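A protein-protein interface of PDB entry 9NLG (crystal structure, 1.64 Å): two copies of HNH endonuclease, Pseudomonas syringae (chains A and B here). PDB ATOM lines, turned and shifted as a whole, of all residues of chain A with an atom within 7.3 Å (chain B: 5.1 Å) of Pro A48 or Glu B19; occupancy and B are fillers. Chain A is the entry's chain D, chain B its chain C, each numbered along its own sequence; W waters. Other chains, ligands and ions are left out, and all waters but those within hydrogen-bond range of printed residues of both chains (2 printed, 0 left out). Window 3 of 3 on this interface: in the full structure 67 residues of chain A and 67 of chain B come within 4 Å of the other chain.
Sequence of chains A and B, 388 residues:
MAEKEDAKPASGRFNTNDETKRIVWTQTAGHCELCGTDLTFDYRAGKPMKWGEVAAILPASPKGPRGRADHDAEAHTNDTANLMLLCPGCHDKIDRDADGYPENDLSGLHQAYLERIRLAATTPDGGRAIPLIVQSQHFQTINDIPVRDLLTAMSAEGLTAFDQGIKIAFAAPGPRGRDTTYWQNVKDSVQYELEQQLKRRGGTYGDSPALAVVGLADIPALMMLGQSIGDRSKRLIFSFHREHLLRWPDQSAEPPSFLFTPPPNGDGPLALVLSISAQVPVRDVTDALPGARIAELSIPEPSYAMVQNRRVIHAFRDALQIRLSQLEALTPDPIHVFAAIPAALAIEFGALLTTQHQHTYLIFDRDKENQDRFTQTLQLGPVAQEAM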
ATOM      1  N   ARG A  22       8.803  29.989 -17.881  1.00  0.00           N
ATOM      2  CA  ARG A  22       9.569  30.820 -18.805  1.00  0.00           C
ATOM      3  C   ARG A  22      10.549  31.714 -18.059  1.00  0.00           C
ATOM      4  O   ARG A  22      11.714  31.837 -18.455  1.00  0.00           O
ATOM      5  CB  ARG A  22       8.619  31.651 -19.671  1.00  0.00           C
ATOM      6  CG  ARG A  22       8.074  30.892 -20.891  1.00  0.00           C
ATOM      7  CD  ARG A  22       6.810  31.533 -21.468  1.00  0.00           C
ATOM      8  NE  ARG A  22       6.067  30.627 -22.343  1.00  0.00           N
ATOM      9  CZ  ARG A  22       6.332  30.428 -23.628  1.00  0.00           C
ATOM     10  NH1 ARG A  22       7.333  31.045 -24.235  1.00  0.00           N
ATOM     11  NH2 ARG A  22       5.576  29.584 -24.324  1.00  0.00           N
ATOM     12  N   THR A  40      18.746  21.141 -20.637  1.00  0.00           N
ATOM     13  CA  THR A  40      18.308  21.157 -22.028  1.00  0.00           C
ATOM     14  C   THR A  40      18.862  19.974 -22.826  1.00  0.00           C
ATOM     15  O   THR A  40      18.754  19.963 -24.059  1.00  0.00           O
ATOM     16  CB  THR A  40      18.705  22.480 -22.701  1.00  0.00           C
ATOM     17  OG1 THR A  40      20.137  22.565 -22.796  1.00  0.00           O
ATOM     18  CG2 THR A  40      18.167  23.683 -21.921  1.00  0.00           C
ATOM     19  N   PHE A  41      19.426  18.970 -22.146  1.00  0.00           N
ATOM     20  CA  PHE A  41      20.080  17.855 -22.830  1.00  0.00           C
ATOM     21  C   PHE A  41      19.186  17.220 -23.892  1.00  0.00           C
ATOM     22  O   PHE A  41      19.668  16.845 -24.969  1.00  0.00           O
ATOM     23  CB  PHE A  41      20.510  16.799 -21.802  1.00  0.00           C
ATOM     24  CG  PHE A  41      19.395  16.347 -20.895  1.00  0.00           C
ATOM     25  CD1 PHE A  41      18.545  15.320 -21.271  1.00  0.00           C
ATOM     26  CD2 PHE A  41      19.202  16.949 -19.664  1.00  0.00           C
ATOM     27  CE1 PHE A  41      17.518  14.909 -20.437  1.00  0.00           C
ATOM     28  CE2 PHE A  41      18.176  16.540 -18.827  1.00  0.00           C
ATOM     29  CZ  PHE A  41      17.337  15.522 -19.214  1.00  0.00           C
ATOM     30  N   ASP A  42      17.888  17.076 -23.614  1.00  0.00           N
ATOM     31  CA  ASP A  42      17.001  16.433 -24.580  1.00  0.00           C
ATOM     32  C   ASP A  42      16.910  17.256 -25.857  1.00  0.00           C
ATOM     33  O   ASP A  42      16.986  16.721 -26.970  1.00  0.00           O
ATOM     34  CB  ASP A  42      15.599  16.235 -24.004  1.00  0.00           C
ATOM     35  CG  ASP A  42      15.477  14.976 -23.173  1.00  0.00           C
ATOM     36  OD1 ASP A  42      16.377  14.112 -23.248  1.00  0.00           O
ATOM     37  OD2 ASP A  42      14.462  14.855 -22.446  1.00  0.00           O
ATOM     38  N   TYR A  43      16.717  18.571 -25.711  1.00  0.00           N
ATOM     39  CA  TYR A  43      16.639  19.429 -26.881  1.00  0.00           C
ATOM     40  C   TYR A  43      17.931  19.362 -27.679  1.00  0.00           C
ATOM     41  O   TYR A  43      17.902  19.327 -28.915  1.00  0.00           O
ATOM     42  CB  TYR A  43      16.322  20.872 -26.476  1.00  0.00           C
ATOM     43  CG  TYR A  43      16.274  21.811 -27.659  1.00  0.00           C
ATOM     44  CD1 TYR A  43      15.100  22.010 -28.373  1.00  0.00           C
ATOM     45  CD2 TYR A  43      17.412  22.489 -28.071  1.00  0.00           C
ATOM     46  CE1 TYR A  43      15.067  22.868 -29.464  1.00  0.00           C
ATOM     47  CE2 TYR A  43      17.391  23.334 -29.149  1.00  0.00           C
ATOM     48  CZ  TYR A  43      16.223  23.527 -29.844  1.00  0.00           C
ATOM     49  OH  TYR A  43      16.221  24.373 -30.919  1.00  0.00           O
ATOM     50  N   ALA A  45      19.809  16.873 -27.993  1.00  0.00           N
ATOM     51  CA  ALA A  45      19.796  15.598 -28.693  1.00  0.00           C
ATOM     52  C   ALA A  45      18.749  15.539 -29.793  1.00  0.00           C
ATOM     53  O   ALA A  45      18.668  14.519 -30.488  1.00  0.00           O
ATOM     54  CB  ALA A  45      19.557  14.454 -27.700  1.00  0.00           C
ATOM     55  N   GLY A  46      17.958  16.594 -29.975  1.00  0.00           N
ATOM     56  CA  GLY A  46      16.943  16.625 -31.005  1.00  0.00           C
ATOM     57  C   GLY A  46      15.574  16.174 -30.563  1.00  0.00           C
ATOM     58  O   GLY A  46      14.694  15.990 -31.413  1.00  0.00           O
ATOM     59  N   LYS A  47      15.363  15.995 -29.272  1.00  0.00           N
ATOM     60  CA  LYS A  47      14.095  15.532 -28.732  1.00  0.00           C
ATOM     61  C   LYS A  47      13.305  16.699 -28.161  1.00  0.00           C
ATOM     62  O   LYS A  47      13.852  17.782 -27.925  1.00  0.00           O
ATOM     63  CB  LYS A  47      14.340  14.477 -27.649  1.00  0.00           C
ATOM     64  CG  LYS A  47      15.510  13.548 -27.972  1.00  0.00           C
ATOM     65  CD  LYS A  47      15.410  12.198 -27.272  1.00  0.00           C
ATOM     66  CE  LYS A  47      15.418  12.322 -25.761  1.00  0.00           C
ATOM     67  NZ  LYS A  47      15.734  11.017 -25.107  1.00  0.00           N
ATOM     68  N   PRO A  48      12.005  16.516 -27.938  1.00  0.00           N
ATOM     69  CA  PRO A  48      11.193  17.602 -27.374  1.00  0.00           C
ATOM     70  C   PRO A  48      11.699  18.024 -26.001  1.00  0.00           C
ATOM     71  O   PRO A  48      12.201  17.216 -25.217  1.00  0.00           O
ATOM     72  CB  PRO A  48       9.788  16.989 -27.288  1.00  0.00           C
ATOM     73  CG  PRO A  48       9.805  15.865 -28.282  1.00  0.00           C
ATOM     74  CD  PRO A  48      11.199  15.319 -28.241  1.00  0.00           C
ATOM     75  N   MET A  49      11.576  19.321 -25.720  1.00  0.00           N
ATOM     76  CA  MET A  49      11.983  19.892 -24.440  1.00  0.00           C
ATOM     77  C   MET A  49      10.817  19.782 -23.464  1.00  0.00           C
ATOM     78  O   MET A  49       9.813  20.483 -23.606  1.00  0.00           O
ATOM     79  CB  MET A  49      12.412  21.346 -24.615  1.00  0.00           C
ATOM     80  CG  MET A  49      13.028  21.964 -23.387  1.00  0.00           C
ATOM     81  SD  MET A  49      14.517  21.089 -22.852  1.00  0.00           S
ATOM     82  CE  MET A  49      14.670  21.739 -21.190  1.00  0.00           C
ATOM     83  N   LYS A  50      10.965  18.919 -22.454  1.00  0.00           N
ATOM     84  CA  LYS A  50       9.909  18.655 -21.476  1.00  0.00           C
ATOM     85  C   LYS A  50      10.241  19.425 -20.200  1.00  0.00           C
ATOM     86  O   LYS A  50      10.717  18.870 -19.205  1.00  0.00           O
ATOM     87  CB  LYS A  50       9.789  17.154 -21.225  1.00  0.00           C
ATOM     88  CG  LYS A  50       9.645  16.340 -22.507  1.00  0.00           C
ATOM     89  CD  LYS A  50       9.431  14.868 -22.213  1.00  0.00           C
ATOM     90  CE  LYS A  50       8.863  14.136 -23.422  1.00  0.00           C
ATOM     91  NZ  LYS A  50       8.645  12.687 -23.130  1.00  0.00           N
ATOM     92  N   TRP A  51       9.971  20.734 -20.239  1.00  0.00           N
ATOM     93  CA  TRP A  51      10.437  21.629 -19.186  1.00  0.00           C
ATOM     94  C   TRP A  51       9.997  21.145 -17.808  1.00  0.00           C
ATOM     95  O   TRP A  51      10.794  21.110 -16.862  1.00  0.00           O
ATOM     96  CB  TRP A  51       9.927  23.060 -19.433  1.00  0.00           C
ATOM     97  CG  TRP A  51      10.080  23.570 -20.857  1.00  0.00           C
ATOM     98  CD1 TRP A  51       9.161  23.467 -21.865  1.00  0.00           C
ATOM     99  CD2 TRP A  51      11.199  24.279 -21.410  1.00  0.00           C
ATOM    100  NE1 TRP A  51       9.645  24.047 -23.012  1.00  0.00           N
ATOM    101  CE2 TRP A  51      10.894  24.557 -22.759  1.00  0.00           C
ATOM    102  CE3 TRP A  51      12.431  24.696 -20.898  1.00  0.00           C
ATOM    103  CZ2 TRP A  51      11.774  25.232 -23.601  1.00  0.00           C
ATOM    104  CZ3 TRP A  51      13.306  25.368 -21.740  1.00  0.00           C
ATOM    105  CH2 TRP A  51      12.970  25.629 -23.077  1.00  0.00           C
ATOM    106  N   VAL A  54      11.954  17.530 -16.835  1.00  0.00           N
ATOM    107  CA  VAL A  54      13.399  17.486 -16.644  1.00  0.00           C
ATOM    108  C   VAL A  54      13.828  18.379 -15.493  1.00  0.00           C
ATOM    109  O   VAL A  54      15.014  18.369 -15.120  1.00  0.00           O
ATOM    110  CB  VAL A  54      14.140  17.875 -17.942  1.00  0.00           C
ATOM    111  CG1 VAL A  54      13.792  16.898 -19.069  1.00  0.00           C
ATOM    112  CG2 VAL A  54      13.824  19.302 -18.357  1.00  0.00           C
ATOM    113  N   ASN B  17      10.339  28.180 -34.306  1.00  0.00           N
ATOM    114  CA  ASN B  17       9.194  27.814 -33.487  1.00  0.00           C
ATOM    115  C   ASN B  17       9.405  28.231 -32.033  1.00  0.00           C
ATOM    116  O   ASN B  17      10.497  28.643 -31.621  1.00  0.00           O
ATOM    117  CB  ASN B  17       8.907  26.309 -33.592  1.00  0.00           C
ATOM    118  CG  ASN B  17      10.084  25.440 -33.172  1.00  0.00           C
ATOM    119  OD1 ASN B  17      10.797  25.740 -32.216  1.00  0.00           O
ATOM    120  ND2 ASN B  17      10.282  24.340 -33.888  1.00  0.00           N
ATOM    121  N   ASP B  18       8.327  28.120 -31.249  1.00  0.00           N
ATOM    122  CA  ASP B  18       8.335  28.621 -29.877  1.00  0.00           C
ATOM    123  C   ASP B  18       9.307  27.841 -29.002  1.00  0.00           C
ATOM    124  O   ASP B  18       9.965  28.422 -28.131  1.00  0.00           O
ATOM    125  CB  ASP B  18       6.918  28.562 -29.295  1.00  0.00           C
ATOM    126  CG  ASP B  18       6.848  29.069 -27.861  1.00  0.00           C
ATOM    127  OD1 ASP B  18       7.311  30.205 -27.603  1.00  0.00           O
ATOM    128  OD2 ASP B  18       6.312  28.339 -26.994  1.00  0.00           O
ATOM    129  N   GLU B  19       9.411  26.524 -29.207  1.00  0.00           N
ATOM    130  CA  GLU B  19      10.364  25.745 -28.425  1.00  0.00           C
ATOM    131  C   GLU B  19      11.777  26.289 -28.596  1.00  0.00           C
ATOM    132  O   GLU B  19      12.527  26.436 -27.620  1.00  0.00           O
ATOM    133  CB  GLU B  19      10.325  24.272 -28.832  1.00  0.00           C
ATOM    134  CG  GLU B  19      11.349  23.420 -28.090  1.00  0.00           C
ATOM    135  CD  GLU B  19      11.361  21.969 -28.544  1.00  0.00           C
ATOM    136  OE1 GLU B  19      11.813  21.698 -29.680  1.00  0.00           O
ATOM    137  OE2 GLU B  19      10.909  21.109 -27.765  1.00  0.00           O
ATOM    138  N   THR B  20      12.161  26.569 -29.840  1.00  0.00           N
ATOM    139  CA  THR B  20      13.511  27.047 -30.111  1.00  0.00           C
ATOM    140  C   THR B  20      13.710  28.453 -29.571  1.00  0.00           C
ATOM    141  O   THR B  20      14.777  28.766 -29.033  1.00  0.00           O
ATOM    142  CB  THR B  20      13.796  27.001 -31.612  1.00  0.00           C
ATOM    143  OG1 THR B  20      13.714  25.644 -32.074  1.00  0.00           O
ATOM    144  CG2 THR B  20      15.184  27.543 -31.915  1.00  0.00           C
ATOM    145  N   LYS B  21      12.701  29.319 -29.705  1.00  0.00           N
ATOM    146  CA  LYS B  21      12.819  30.645 -29.104  1.00  0.00           C
ATOM    147  C   LYS B  21      12.982  30.539 -27.594  1.00  0.00           C
ATOM    148  O   LYS B  21      13.795  31.254 -26.994  1.00  0.00           O
ATOM    149  CB  LYS B  21      11.605  31.501 -29.465  1.00  0.00           C
ATOM    150  CG  LYS B  21      11.610  31.960 -30.917  1.00  0.00           C
ATOM    151  CD  LYS B  21      10.330  32.694 -31.300  1.00  0.00           C
ATOM    152  CE  LYS B  21      10.436  33.296 -32.695  1.00  0.00           C
ATOM    153  NZ  LYS B  21      11.113  34.626 -32.674  1.00  0.00           N
ATOM    154  N   ARG B  22      12.243  29.624 -26.959  1.00  0.00           N
ATOM    155  CA  ARG B  22      12.401  29.439 -25.522  1.00  0.00           C
ATOM    156  C   ARG B  22      13.813  28.981 -25.183  1.00  0.00           C
ATOM    157  O   ARG B  22      14.384  29.409 -24.174  1.00  0.00           O
ATOM    158  CB  ARG B  22      11.379  28.437 -24.992  1.00  0.00           C
ATOM    159  CG  ARG B  22       9.963  28.978 -24.910  1.00  0.00           C
ATOM    160  CD  ARG B  22       9.002  27.928 -24.364  1.00  0.00           C
ATOM    161  NE  ARG B  22       9.166  27.736 -22.927  1.00  0.00           N
ATOM    162  CZ  ARG B  22       8.325  27.056 -22.158  1.00  0.00           C
ATOM    163  NH1 ARG B  22       7.251  26.471 -22.662  1.00  0.00           N
ATOM    164  NH2 ARG B  22       8.566  26.966 -20.853  1.00  0.00           N
ATOM    165  N   ILE B  23      14.388  28.103 -26.006  1.00  0.00           N
ATOM    166  CA  ILE B  23      15.752  27.652 -25.752  1.00  0.00           C
ATOM    167  C   ILE B  23      16.731  28.807 -25.919  1.00  0.00           C
ATOM    168  O   ILE B  23      17.673  28.955 -25.130  1.00  0.00           O
ATOM    169  CB  ILE B  23      16.107  26.468 -26.669  1.00  0.00           C
ATOM    170  CG1 ILE B  23      15.368  25.200 -26.221  1.00  0.00           C
ATOM    171  CG2 ILE B  23      17.604  26.236 -26.691  1.00  0.00           C
ATOM    172  CD1 ILE B  23      15.924  24.550 -24.943  1.00  0.00           C
HETATM  173  O   HOH W   1       8.868  21.534 -26.052  1.00  0.00           O
HETATM  174  O   HOH W   2      13.375  19.475 -30.125  1.00  0.00           O
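NH2 of Arg A22 lies within salt-bridge range of OD2 of Asp B18 (3.0 Å).
N of Met A49 is in hydrogen-bond range of OE2 of Glu B19 (2.8 Å).
The side-chain hydroxyl (OG1) of Thr B20 lies within hydrogen-bond range of the side-chain hydroxyl (OH) of Tyr A43 (3.0 Å).
NE1 of Trp A51 lies close to NH1 of Arg B22.
OD1 of Asn B17 lies close to N of Glu B19.
The side-chain amide oxygen (OD1) of Asn B17 is in hydrogen-bond range of the backbone NH (N) of Thr B20, 2.9 Å away.
Arg A22 touches Arg B22 (NH1 to CG, 3.4 Å).
CD1 of Ile B23 touches CG2 of Thr A40, 3.9 Å away.
Tyr A43 touches Glu B19.
CG1 of Ile B23 touches CG of Tyr A43 (3.8 Å).
Pro A48 touches Glu B19 (CA to OE2, 3.5 Å).
Trp A51 touches Ile B23.
Gly A46 touches none of the printed residues of chain B.
Pro A48 touches just one residue of chain B: Glu B19 (3.5 Å).
Lys A50 touches none of the printed residues of chain B.
Of the printed residues of chain A, Asp B18 touches Arg A22.
Glu B19 touches just these residues of chain A: Tyr A43 (3.5 Å), Pro A48 (3.5 Å) and Met A49 (2.8 Å).
Of the printed residues of chain A, Ile B23 touches Thr A40, Tyr A43 and Trp A51.
The nearest printed residue of chain B that does not touch Pro A48 is Ile B23 (7.8 Å).
The nearest residue of chain A that does not touch Glu B19 is Trp A51 (4.3 Å).
Of the 7 printed residues of chain B, 5 touch a printed residue of chain A.
Printed residues of chain B that touch a printed residue of chain A: Asp B18, Glu B19, Thr B20, Arg B22 and Ile B23.
Along chain B the printed residues that touch a printed residue of chain A span positions 18 to 23.
Printed residues of chain A that touch a printed residue of chain B: Arg A22, Thr A40, Tyr A43, Pro A48, Met A49 and Trp A51.
Hydrophobic or aromatic side chains of chain A that line the printed part of chain B: Tyr A43, Met A49 and Trp A51.
Among the printed residues, 10 pairs touch across the chains.
Arg A22 touches its own counterpart, Arg B22.
Of the 10 pairs that touch across the chains among the printed residues, 1 has its exchanged pair printed and touching as well.
Water W1 bridges OE2 of Glu B19 (2.7 Å) and O of Met A49 (2.8 Å).
Water W2 lies within hydrogen-bond range of the side-chain carboxylate (OE1) of Glu B19 (2.8 Å) and the backbone carbonyl oxygen (O) of Lys A47 (2.8 Å).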
